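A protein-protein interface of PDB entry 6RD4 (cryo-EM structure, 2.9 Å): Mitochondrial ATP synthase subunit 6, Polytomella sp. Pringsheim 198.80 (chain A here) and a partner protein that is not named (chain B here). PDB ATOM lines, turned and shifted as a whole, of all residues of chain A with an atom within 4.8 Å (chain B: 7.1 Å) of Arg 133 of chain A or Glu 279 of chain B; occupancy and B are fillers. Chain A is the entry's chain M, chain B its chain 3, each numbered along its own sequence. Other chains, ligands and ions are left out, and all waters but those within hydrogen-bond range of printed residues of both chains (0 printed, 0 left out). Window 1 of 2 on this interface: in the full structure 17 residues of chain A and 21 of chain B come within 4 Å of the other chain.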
ATOM      1  N   ASN A 131      -1.740  -0.564   4.721  1.00  0.00           N
ATOM      2  CA  ASN A 131      -2.370   0.741   4.642  1.00  0.00           C
ATOM      3  C   ASN A 131      -1.574   1.525   3.612  1.00  0.00           C
ATOM      4  O   ASN A 131      -0.793   0.943   2.860  1.00  0.00           O
ATOM      5  CB  ASN A 131      -2.443   1.375   6.032  1.00  0.00           C
ATOM      6  CG  ASN A 131      -1.142   1.280   6.789  1.00  0.00           C
ATOM      7  OD1 ASN A 131      -0.110   0.918   6.244  1.00  0.00           O
ATOM      8  ND2 ASN A 131      -1.198   1.571   8.074  1.00  0.00           N
ATOM      9  N   ASP A 132      -1.740   2.847   3.567  1.00  0.00           N
ATOM     10  CA  ASP A 132      -1.022   3.649   2.579  1.00  0.00           C
ATOM     11  C   ASP A 132       0.475   3.702   2.820  1.00  0.00           C
ATOM     12  O   ASP A 132       1.211   4.140   1.937  1.00  0.00           O
ATOM     13  CB  ASP A 132      -1.537   5.080   2.550  1.00  0.00           C
ATOM     14  CG  ASP A 132      -2.915   5.196   1.970  1.00  0.00           C
ATOM     15  OD1 ASP A 132      -3.886   5.198   2.751  1.00  0.00           O
ATOM     16  OD2 ASP A 132      -3.028   5.310   0.735  1.00  0.00           O
ATOM     17  N   ARG A 133       0.937   3.314   3.997  1.00  0.00           N
ATOM     18  CA  ARG A 133       2.362   3.174   4.221  1.00  0.00           C
ATOM     19  C   ARG A 133       2.896   1.947   3.504  1.00  0.00           C
ATOM     20  O   ARG A 133       3.934   2.009   2.845  1.00  0.00           O
ATOM     21  CB  ARG A 133       2.633   3.083   5.717  1.00  0.00           C
ATOM     22  CG  ARG A 133       4.079   2.934   6.089  1.00  0.00           C
ATOM     23  CD  ARG A 133       4.806   4.245   6.054  1.00  0.00           C
ATOM     24  NE  ARG A 133       6.225   4.029   6.261  1.00  0.00           N
ATOM     25  CZ  ARG A 133       7.095   3.919   5.274  1.00  0.00           C
ATOM     26  NH1 ARG A 133       6.680   4.027   4.031  1.00  0.00           N
ATOM     27  NH2 ARG A 133       8.371   3.714   5.524  1.00  0.00           N
ATOM     28  N   LEU A 134       2.175   0.844   3.592  1.00  0.00           N
ATOM     29  CA  LEU A 134       2.631  -0.427   3.067  1.00  0.00           C
ATOM     30  C   LEU A 134       2.205  -0.658   1.629  1.00  0.00           C
ATOM     31  O   LEU A 134       2.565  -1.677   1.048  1.00  0.00           O
ATOM     32  CB  LEU A 134       2.100  -1.544   3.950  1.00  0.00           C
ATOM     33  CG  LEU A 134       2.939  -2.798   4.049  1.00  0.00           C
ATOM     34  CD1 LEU A 134       4.198  -2.448   4.734  1.00  0.00           C
ATOM     35  CD2 LEU A 134       2.211  -3.853   4.800  1.00  0.00           C
ATOM     36  N   LEU A 135       1.455   0.259   1.037  1.00  0.00           N
ATOM     37  CA  LEU A 135       0.944   0.030  -0.308  1.00  0.00           C
ATOM     38  C   LEU A 135       2.001   0.051  -1.399  1.00  0.00           C
ATOM     39  O   LEU A 135       1.850  -0.731  -2.349  1.00  0.00           O
ATOM     40  CB  LEU A 135      -0.166   1.025  -0.641  1.00  0.00           C
ATOM     41  CG  LEU A 135      -1.599   0.605  -0.395  1.00  0.00           C
ATOM     42  CD1 LEU A 135      -2.469   1.658  -0.982  1.00  0.00           C
ATOM     43  CD2 LEU A 135      -1.881  -0.739  -0.989  1.00  0.00           C
ATOM     44  N   PRO A 136       3.048   0.885  -1.382  1.00  0.00           N
ATOM     45  CA  PRO A 136       4.107   0.673  -2.370  1.00  0.00           C
ATOM     46  C   PRO A 136       4.926  -0.560  -2.137  1.00  0.00           C
ATOM     47  O   PRO A 136       5.540  -1.046  -3.082  1.00  0.00           O
ATOM     48  CB  PRO A 136       4.964   1.924  -2.238  1.00  0.00           C
ATOM     49  CG  PRO A 136       4.091   2.880  -1.774  1.00  0.00           C
ATOM     50  CD  PRO A 136       3.191   2.237  -0.825  1.00  0.00           C
ATOM     51  N   PRO A 318       8.609  -0.823   5.561  1.00  0.00           N
ATOM     52  CA  PRO A 318       9.036   0.437   6.176  1.00  0.00           C
ATOM     53  C   PRO A 318      10.384   0.295   6.867  1.00  0.00           C
ATOM     54  O   PRO A 318      10.575  -0.573   7.719  1.00  0.00           O
ATOM     55  CB  PRO A 318       7.925   0.735   7.185  1.00  0.00           C
ATOM     56  CG  PRO A 318       7.290  -0.565   7.442  1.00  0.00           C
ATOM     57  CD  PRO A 318       7.408  -1.366   6.201  1.00  0.00           C
ATOM     58  N   ALA A 319      11.321   1.155   6.485  1.00  0.00           N
ATOM     59  CA  ALA A 319      12.608   1.229   7.154  1.00  0.00           C
ATOM     60  C   ALA A 319      12.620   2.216   8.306  1.00  0.00           C
ATOM     61  O   ALA A 319      13.569   2.219   9.091  1.00  0.00           O
ATOM     62  CB  ALA A 319      13.700   1.615   6.159  1.00  0.00           C
ATOM     63  N   ALA A 320      11.599   3.055   8.430  1.00  0.00           N
ATOM     64  CA  ALA A 320      11.505   4.003   9.521  1.00  0.00           C
ATOM     65  C   ALA A 320      10.047   4.188   9.892  1.00  0.00           C
ATOM     66  O   ALA A 320       9.179   4.245   9.026  1.00  0.00           O
ATOM     67  CB  ALA A 320      12.129   5.333   9.145  1.00  0.00           C
ATOM     68  N   LYS A 321       9.786   4.299  11.184  1.00  0.00           N
ATOM     69  CA  LYS A 321       8.425   4.276  11.685  1.00  0.00           C
ATOM     70  C   LYS A 321       8.241   5.394  12.697  1.00  0.00           C
ATOM     71  O   LYS A 321       9.207   5.958  13.207  1.00  0.00           O
ATOM     72  CB  LYS A 321       8.102   2.923  12.319  1.00  0.00           C
ATOM     73  CG  LYS A 321       6.660   2.510  12.202  1.00  0.00           C
ATOM     74  CD  LYS A 321       6.307   1.429  13.192  1.00  0.00           C
ATOM     75  CE  LYS A 321       7.004   0.133  12.864  1.00  0.00           C
ATOM     76  NZ  LYS A 321       6.592  -0.943  13.801  1.00  0.00           N
ATOM     77  N   ILE A 322       6.986   5.739  12.950  1.00  0.00           N
ATOM     78  CA  ILE A 322       6.597   6.609  14.051  1.00  0.00           C
ATOM     79  C   ILE A 322       5.610   5.799  14.881  1.00  0.00           C
ATOM     80  O   ILE A 322       4.419   5.715  14.562  1.00  0.00           O
ATOM     81  CB  ILE A 322       6.014   7.938  13.560  1.00  0.00           C
ATOM     82  CG1 ILE A 322       7.111   8.720  12.851  1.00  0.00           C
ATOM     83  CG2 ILE A 322       5.455   8.765  14.685  1.00  0.00           C
ATOM     84  CD1 ILE A 322       6.714  10.057  12.381  1.00  0.00           C
ATOM     85  N   ALA B 241       1.428  11.439  -1.404  1.00  0.00           N
ATOM     86  CA  ALA B 241       2.178  10.822  -0.326  1.00  0.00           C
ATOM     87  C   ALA B 241       2.193   9.306  -0.381  1.00  0.00           C
ATOM     88  O   ALA B 241       2.977   8.704   0.348  1.00  0.00           O
ATOM     89  CB  ALA B 241       1.617  11.239   1.016  1.00  0.00           C
ATOM     90  N   ARG B 242       1.339   8.670  -1.182  1.00  0.00           N
ATOM     91  CA  ARG B 242       1.491   7.239  -1.413  1.00  0.00           C
ATOM     92  C   ARG B 242       2.761   6.948  -2.170  1.00  0.00           C
ATOM     93  O   ARG B 242       3.435   5.961  -1.899  1.00  0.00           O
ATOM     94  CB  ARG B 242       0.316   6.689  -2.196  1.00  0.00           C
ATOM     95  CG  ARG B 242      -0.900   6.583  -1.400  1.00  0.00           C
ATOM     96  CD  ARG B 242      -2.075   6.481  -2.284  1.00  0.00           C
ATOM     97  NE  ARG B 242      -3.218   6.756  -1.458  1.00  0.00           N
ATOM     98  CZ  ARG B 242      -4.339   7.261  -1.919  1.00  0.00           C
ATOM     99  NH1 ARG B 242      -5.336   7.504  -1.097  1.00  0.00           N
ATOM    100  NH2 ARG B 242      -4.424   7.588  -3.190  1.00  0.00           N
ATOM    101  N   PHE B 244       5.683   7.975  -2.031  1.00  0.00           N
ATOM    102  CA  PHE B 244       6.936   8.109  -1.309  1.00  0.00           C
ATOM    103  C   PHE B 244       7.080   6.900  -0.415  1.00  0.00           C
ATOM    104  O   PHE B 244       6.283   6.709   0.504  1.00  0.00           O
ATOM    105  CB  PHE B 244       6.968   9.385  -0.482  1.00  0.00           C
ATOM    106  CG  PHE B 244       7.061  10.613  -1.298  1.00  0.00           C
ATOM    107  CD1 PHE B 244       8.186  10.867  -2.035  1.00  0.00           C
ATOM    108  CD2 PHE B 244       6.023  11.501  -1.342  1.00  0.00           C
ATOM    109  CE1 PHE B 244       8.277  11.989  -2.795  1.00  0.00           C
ATOM    110  CE2 PHE B 244       6.114  12.619  -2.101  1.00  0.00           C
ATOM    111  CZ  PHE B 244       7.240  12.861  -2.831  1.00  0.00           C
ATOM    112  N   SER B 245       8.080   6.081  -0.693  1.00  0.00           N
ATOM    113  CA  SER B 245       8.356   4.932   0.138  1.00  0.00           C
ATOM    114  C   SER B 245       9.834   4.618   0.022  1.00  0.00           C
ATOM    115  O   SER B 245      10.588   5.339  -0.632  1.00  0.00           O
ATOM    116  CB  SER B 245       7.488   3.741  -0.264  1.00  0.00           C
ATOM    117  OG  SER B 245       7.758   2.627   0.561  1.00  0.00           O
ATOM    118  N   GLU B 246      10.252   3.538   0.673  1.00  0.00           N
ATOM    119  CA  GLU B 246      11.604   3.044   0.489  1.00  0.00           C
ATOM    120  C   GLU B 246      11.817   2.543  -0.922  1.00  0.00           C
ATOM    121  O   GLU B 246      12.933   2.610  -1.443  1.00  0.00           O
ATOM    122  CB  GLU B 246      11.879   1.922   1.475  1.00  0.00           C
ATOM    123  CG  GLU B 246      12.053   2.383   2.888  1.00  0.00           C
ATOM    124  CD  GLU B 246      10.747   2.517   3.625  1.00  0.00           C
ATOM    125  OE1 GLU B 246       9.693   2.232   3.027  1.00  0.00           O
ATOM    126  OE2 GLU B 246      10.770   2.918   4.804  1.00  0.00           O
ATOM    127  N   LEU B 265      10.097  17.459   1.826  1.00  0.00           N
ATOM    128  CA  LEU B 265       9.834  17.886   3.192  1.00  0.00           C
ATOM    129  C   LEU B 265       9.574  19.379   3.266  1.00  0.00           C
ATOM    130  O   LEU B 265       8.872  19.843   4.168  1.00  0.00           O
ATOM    131  CB  LEU B 265      11.000  17.512   4.097  1.00  0.00           C
ATOM    132  CG  LEU B 265      11.192  16.026   4.343  1.00  0.00           C
ATOM    133  CD1 LEU B 265      12.354  15.794   5.252  1.00  0.00           C
ATOM    134  CD2 LEU B 265       9.951  15.434   4.934  1.00  0.00           C
ATOM    135  N   PRO B 275       1.530  13.047   6.579  1.00  0.00           N
ATOM    136  CA  PRO B 275       0.889  11.748   6.430  1.00  0.00           C
ATOM    137  C   PRO B 275       1.747  10.663   7.048  1.00  0.00           C
ATOM    138  O   PRO B 275       2.892  10.883   7.421  1.00  0.00           O
ATOM    139  CB  PRO B 275       0.829  11.594   4.924  1.00  0.00           C
ATOM    140  CG  PRO B 275       2.031  12.262   4.484  1.00  0.00           C
ATOM    141  CD  PRO B 275       2.202  13.445   5.339  1.00  0.00           C
ATOM    142  N   GLU B 276       1.185   9.459   7.112  1.00  0.00           N
ATOM    143  CA  GLU B 276       1.923   8.361   7.713  1.00  0.00           C
ATOM    144  C   GLU B 276       3.069   7.894   6.844  1.00  0.00           C
ATOM    145  O   GLU B 276       3.918   7.150   7.321  1.00  0.00           O
ATOM    146  CB  GLU B 276       1.004   7.182   8.002  1.00  0.00           C
ATOM    147  CG  GLU B 276       1.415   6.356   9.204  1.00  0.00           C
ATOM    148  CD  GLU B 276       0.778   4.993   9.212  1.00  0.00           C
ATOM    149  OE1 GLU B 276       0.044   4.683   8.256  1.00  0.00           O
ATOM    150  OE2 GLU B 276       1.010   4.225  10.166  1.00  0.00           O
ATOM    151  N   SER B 277       3.104   8.288   5.580  1.00  0.00           N
ATOM    152  CA  SER B 277       4.218   7.975   4.707  1.00  0.00           C
ATOM    153  C   SER B 277       5.174   9.133   4.579  1.00  0.00           C
ATOM    154  O   SER B 277       5.879   9.231   3.576  1.00  0.00           O
ATOM    155  CB  SER B 277       3.717   7.574   3.331  1.00  0.00           C
ATOM    156  OG  SER B 277       3.349   8.720   2.603  1.00  0.00           O
ATOM    157  N   ILE B 278       5.179  10.048   5.551  1.00  0.00           N
ATOM    158  CA  ILE B 278       6.285  10.995   5.648  1.00  0.00           C
ATOM    159  C   ILE B 278       7.454  10.355   6.364  1.00  0.00           C
ATOM    160  O   ILE B 278       8.589  10.809   6.220  1.00  0.00           O
ATOM    161  CB  ILE B 278       5.859  12.307   6.337  1.00  0.00           C
ATOM    162  CG1 ILE B 278       6.753  13.453   5.886  1.00  0.00           C
ATOM    163  CG2 ILE B 278       5.901  12.199   7.836  1.00  0.00           C
ATOM    164  CD1 ILE B 278       6.284  14.778   6.343  1.00  0.00           C
ATOM    165  N   GLU B 279       7.229   9.251   7.054  1.00  0.00           N
ATOM    166  CA  GLU B 279       8.306   8.570   7.740  1.00  0.00           C
ATOM    167  C   GLU B 279       9.156   7.723   6.811  1.00  0.00           C
ATOM    168  O   GLU B 279      10.013   6.984   7.286  1.00  0.00           O
ATOM    169  CB  GLU B 279       7.723   7.731   8.860  1.00  0.00           C
ATOM    170  CG  GLU B 279       6.914   6.586   8.403  1.00  0.00           C
ATOM    171  CD  GLU B 279       5.930   6.148   9.442  1.00  0.00           C
ATOM    172  OE1 GLU B 279       5.742   6.889  10.412  1.00  0.00           O
ATOM    173  OE2 GLU B 279       5.343   5.060   9.307  1.00  0.00           O
ATOM    174  N   ALA B 280       8.933   7.791   5.507  1.00  0.00           N
ATOM    175  CA  ALA B 280       9.807   7.180   4.525  1.00  0.00           C
ATOM    176  C   ALA B 280      10.644   8.190   3.776  1.00  0.00           C
ATOM    177  O   ALA B 280      11.625   7.803   3.139  1.00  0.00           O
ATOM    178  CB  ALA B 280       8.991   6.396   3.510  1.00  0.00           C
ATOM    179  N   VAL B 281      10.259   9.460   3.802  1.00  0.00           N
ATOM    180  CA  VAL B 281      11.036  10.497   3.145  1.00  0.00           C
ATOM    181  C   VAL B 281      11.920  11.129   4.213  1.00  0.00           C
ATOM    182  O   VAL B 281      13.031  11.577   3.923  1.00  0.00           O
ATOM    183  CB  VAL B 281      10.121  11.499   2.408  1.00  0.00           C
ATOM    184  CG1 VAL B 281       9.104  12.092   3.309  1.00  0.00           C
ATOM    185  CG2 VAL B 281      10.892  12.579   1.719  1.00  0.00           C
ATOM    186  N   ILE B 282      11.472  11.105   5.468  1.00  0.00           N
ATOM    187  CA  ILE B 282      12.363  11.481   6.562  1.00  0.00           C
ATOM    188  C   ILE B 282      13.421  10.412   6.764  1.00  0.00           C
ATOM    189  O   ILE B 282      14.619  10.701   6.785  1.00  0.00           O
ATOM    190  CB  ILE B 282      11.573  11.725   7.857  1.00  0.00           C
ATOM    191  CG1 ILE B 282      10.664  12.930   7.719  1.00  0.00           C
ATOM    192  CG2 ILE B 282      12.510  12.000   8.971  1.00  0.00           C
ATOM    193  CD1 ILE B 282       9.721  13.057   8.867  1.00  0.00           C
ATOM    194  N   GLY B 283      13.003   9.150   6.846  1.00  0.00           N
ATOM    195  CA  GLY B 283      13.924   8.045   7.020  1.00  0.00           C
ATOM    196  C   GLY B 283      14.827   7.780   5.835  1.00  0.00           C
ATOM    197  O   GLY B 283      15.731   6.953   5.941  1.00  0.00           O
ATOM    198  N   ALA B 284      14.581   8.424   4.700  1.00  0.00           N
ATOM    199  CA  ALA B 284      15.518   8.371   3.593  1.00  0.00           C
ATOM    200  C   ALA B 284      16.672   9.326   3.784  1.00  0.00           C
ATOM    201  O   ALA B 284      17.691   9.192   3.099  1.00  0.00           O
ATOM    202  CB  ALA B 284      14.824   8.707   2.280  1.00  0.00           C
ATOM    203  N   ALA B 307       6.174  16.354  12.467  1.00  0.00           N
ATOM    204  CA  ALA B 307       5.404  15.188  12.073  1.00  0.00           C
ATOM    205  C   ALA B 307       5.215  14.202  13.206  1.00  0.00           C
ATOM    206  O   ALA B 307       4.326  13.356  13.125  1.00  0.00           O
ATOM    207  CB  ALA B 307       6.088  14.484  10.908  1.00  0.00           C
ATOM    208  N   LEU B 311       1.461  12.755  13.988  1.00  0.00           N
ATOM    209  CA  LEU B 311       1.180  11.332  13.930  1.00  0.00           C
ATOM    210  C   LEU B 311       1.073  10.697  15.305  1.00  0.00           C
ATOM    211  O   LEU B 311       0.613   9.558  15.406  1.00  0.00           O
ATOM    212  CB  LEU B 311       2.257  10.645  13.105  1.00  0.00           C
ATOM    213  CG  LEU B 311       2.077  10.931  11.619  1.00  0.00           C
ATOM    214  CD1 LEU B 311       3.372  10.857  10.849  1.00  0.00           C
ATOM    215  CD2 LEU B 311       1.090   9.934  11.083  1.00  0.00           C
ATOM    216  N   GLU B 314       6.893   8.851  18.250  1.00  0.00           N
ATOM    217  CA  GLU B 314       8.277   9.247  18.065  1.00  0.00           C
ATOM    218  C   GLU B 314       8.920   8.435  16.949  1.00  0.00           C
ATOM    219  O   GLU B 314       8.618   7.257  16.746  1.00  0.00           O
ATOM    220  CB  GLU B 314       9.086   9.119  19.371  1.00  0.00           C
ATOM    221  CG  GLU B 314       9.386   7.709  19.854  1.00  0.00           C
ATOM    222  CD  GLU B 314       8.307   7.143  20.752  1.00  0.00           C
ATOM    223  OE1 GLU B 314       7.183   7.683  20.757  1.00  0.00           O
ATOM    224  OE2 GLU B 314       8.590   6.161  21.468  1.00  0.00           O
ATOM    225  N   PHE B 315       9.808   9.106  16.226  1.00  0.00           N
ATOM    226  CA  PHE B 315      10.496   8.511  15.096  1.00  0.00           C
ATOM    227  C   PHE B 315      11.493   7.466  15.558  1.00  0.00           C
ATOM    228  O   PHE B 315      12.175   7.644  16.567  1.00  0.00           O
ATOM    229  CB  PHE B 315      11.225   9.599  14.333  1.00  0.00           C
ATOM    230  CG  PHE B 315      11.463   9.285  12.914  1.00  0.00           C
ATOM    231  CD1 PHE B 315      10.526   9.624  11.963  1.00  0.00           C
ATOM    232  CD2 PHE B 315      12.631   8.678  12.519  1.00  0.00           C
ATOM    233  CE1 PHE B 315      10.741   9.349  10.650  1.00  0.00           C
ATOM    234  CE2 PHE B 315      12.851   8.404  11.207  1.00  0.00           C
ATOM    235  CZ  PHE B 315      11.909   8.735  10.271  1.00  0.00           C
ATOM    236  N   VAL B 316      11.592   6.375  14.810  1.00  0.00           N
ATOM    237  CA  VAL B 316      12.563   5.330  15.102  1.00  0.00           C
ATOM    238  C   VAL B 316      12.935   4.616  13.811  1.00  0.00           C
ATOM    239  O   VAL B 316      12.083   4.025  13.146  1.00  0.00           O
ATOM    240  CB  VAL B 316      12.042   4.355  16.184  1.00  0.00           C
ATOM    241  CG1 VAL B 316      10.604   3.960  15.958  1.00  0.00           C
ATOM    242  CG2 VAL B 316      12.908   3.126  16.261  1.00  0.00           C
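NE of Arg 242 of chain B is in salt-bridge range of OD2 of Asp 132 of chain A, 2.6 Å away. O of Lys 321 of chain A is in hydrogen-bond range of N of Val 316 of chain B, at 2.9 Å. ND2 of Asn 131 of chain A sits at hydrogen-bond distance from OE1 of Glu 276 of chain B. The side-chain carboxylate of Glu 279 of chain B is in hydrogen-bond range of the backbone NH of Ile 322 of chain A (3.1 Å). NE of Arg 133 of chain A lies within salt-bridge range of OE2 of Glu 279 of chain B, at 3.3 Å. The backbone NH (N) of Ala 319 of chain A sits at hydrogen-bond distance from the side-chain carboxylate (OE2) of Glu 246 of chain B. The backbone carbonyl oxygen of Glu 279 of chain B lies close to the backbone carbonyl oxygen of Ala 320 of chain A, at 3.4 Å. OE2 of Glu 246 of chain B is in salt-bridge range of NH2 of Arg 133 of chain A.
OD1 of Asn 131 of chain A lies close to N of Arg 133 of chain A (3.4 Å). The side-chain carboxylate of Glu 246 of chain B lies within hydrogen-bond range of the side-chain hydroxyl of Ser 245 of chain B, 3.2 Å away.
Among the printed residues, pairs that only touch across the chains: Pro 136 of chain A with Arg 242 of chain B (3.2 Å), Arg 133 of chain A with Glu 276 of chain B (3.3 Å), Pro 318 of chain A with Glu 246 of chain B (3.3 Å), Arg 133 of chain A with Ala 280 of chain B (3.4 Å), Lys 321 of chain A with Phe 315 of chain B (3.4 Å), Ile 322 of chain A with Glu 314 of chain B (3.4 Å), Ala 320 of chain A with Phe 315 of chain B (3.6 Å), Ile 322 of chain A with Phe 315 of chain B (3.6 Å), Ala 320 of chain A with Val 316 of chain B (3.7 Å), Pro 136 of chain A with Ser 245 of chain B (3.7 Å), Lys 321 of chain A with Glu 279 of chain B (3.7 Å), Ala 320 of chain A with Glu 246 of chain B (3.7 Å), Ile 322 of chain A with Leu 311 of chain B (3.8 Å), Lys 321 of chain A with Glu 314 of chain B (3.8 Å), Ala 320 of chain A with Gly 283 of chain B (3.9 Å) and Arg 133 of chain A with Ser 245 of chain B (3.9 Å).
Printed residues of chain B within 4 Å of Arg 133 of chain A: Ser 245, Glu 246, Glu 276, Glu 279 and Ala 280. Glu 279 of chain B touches just these residues of chain A: Arg 133, Ala 320, Lys 321 and Ile 322. Printed residues of chain A within 4 Å of Phe 315 of chain B: Ala 320, Lys 321 and Ile 322. Printed residues of chain A within 4 Å of Glu 314 of chain B: Lys 321 (3.8 Å) and Ile 322 (3.4 Å). Printed residues of chain B within 4 Å of Pro 136 of chain A: Arg 242 and Ser 245. Pro 275 of chain B touches none of the printed residues of chain A. Leu 265 of chain B touches none of the printed residues of chain A.
Of the 21 printed residues of chain B, 11 touch a printed residue of chain A. Of the 11 printed residues of chain A, 9 touch a printed residue of chain B. Printed residues of chain A that touch a printed residue of chain B: Asn 131, Asp 132, Arg 133, Pro 136, Pro 318, Ala 319, Ala 320, Lys 321 and Ile 322. Hydrophobic or aromatic side chains of chain A that line the printed part of chain B: Pro 136, Ala 319, Ala 320 and Ile 322. Among the printed residues, 24 pairs touch across the chains. Among the printed residues, Asp or Glu carboxylates within 4 Å of a Lys or Arg side-chain nitrogen of the other chain: Asp 132 of chain A with Arg 242 of chain B, Arg 133 of chain A with Glu 246 of chain B and Arg 133 of chain A with Glu 279 of chain B.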
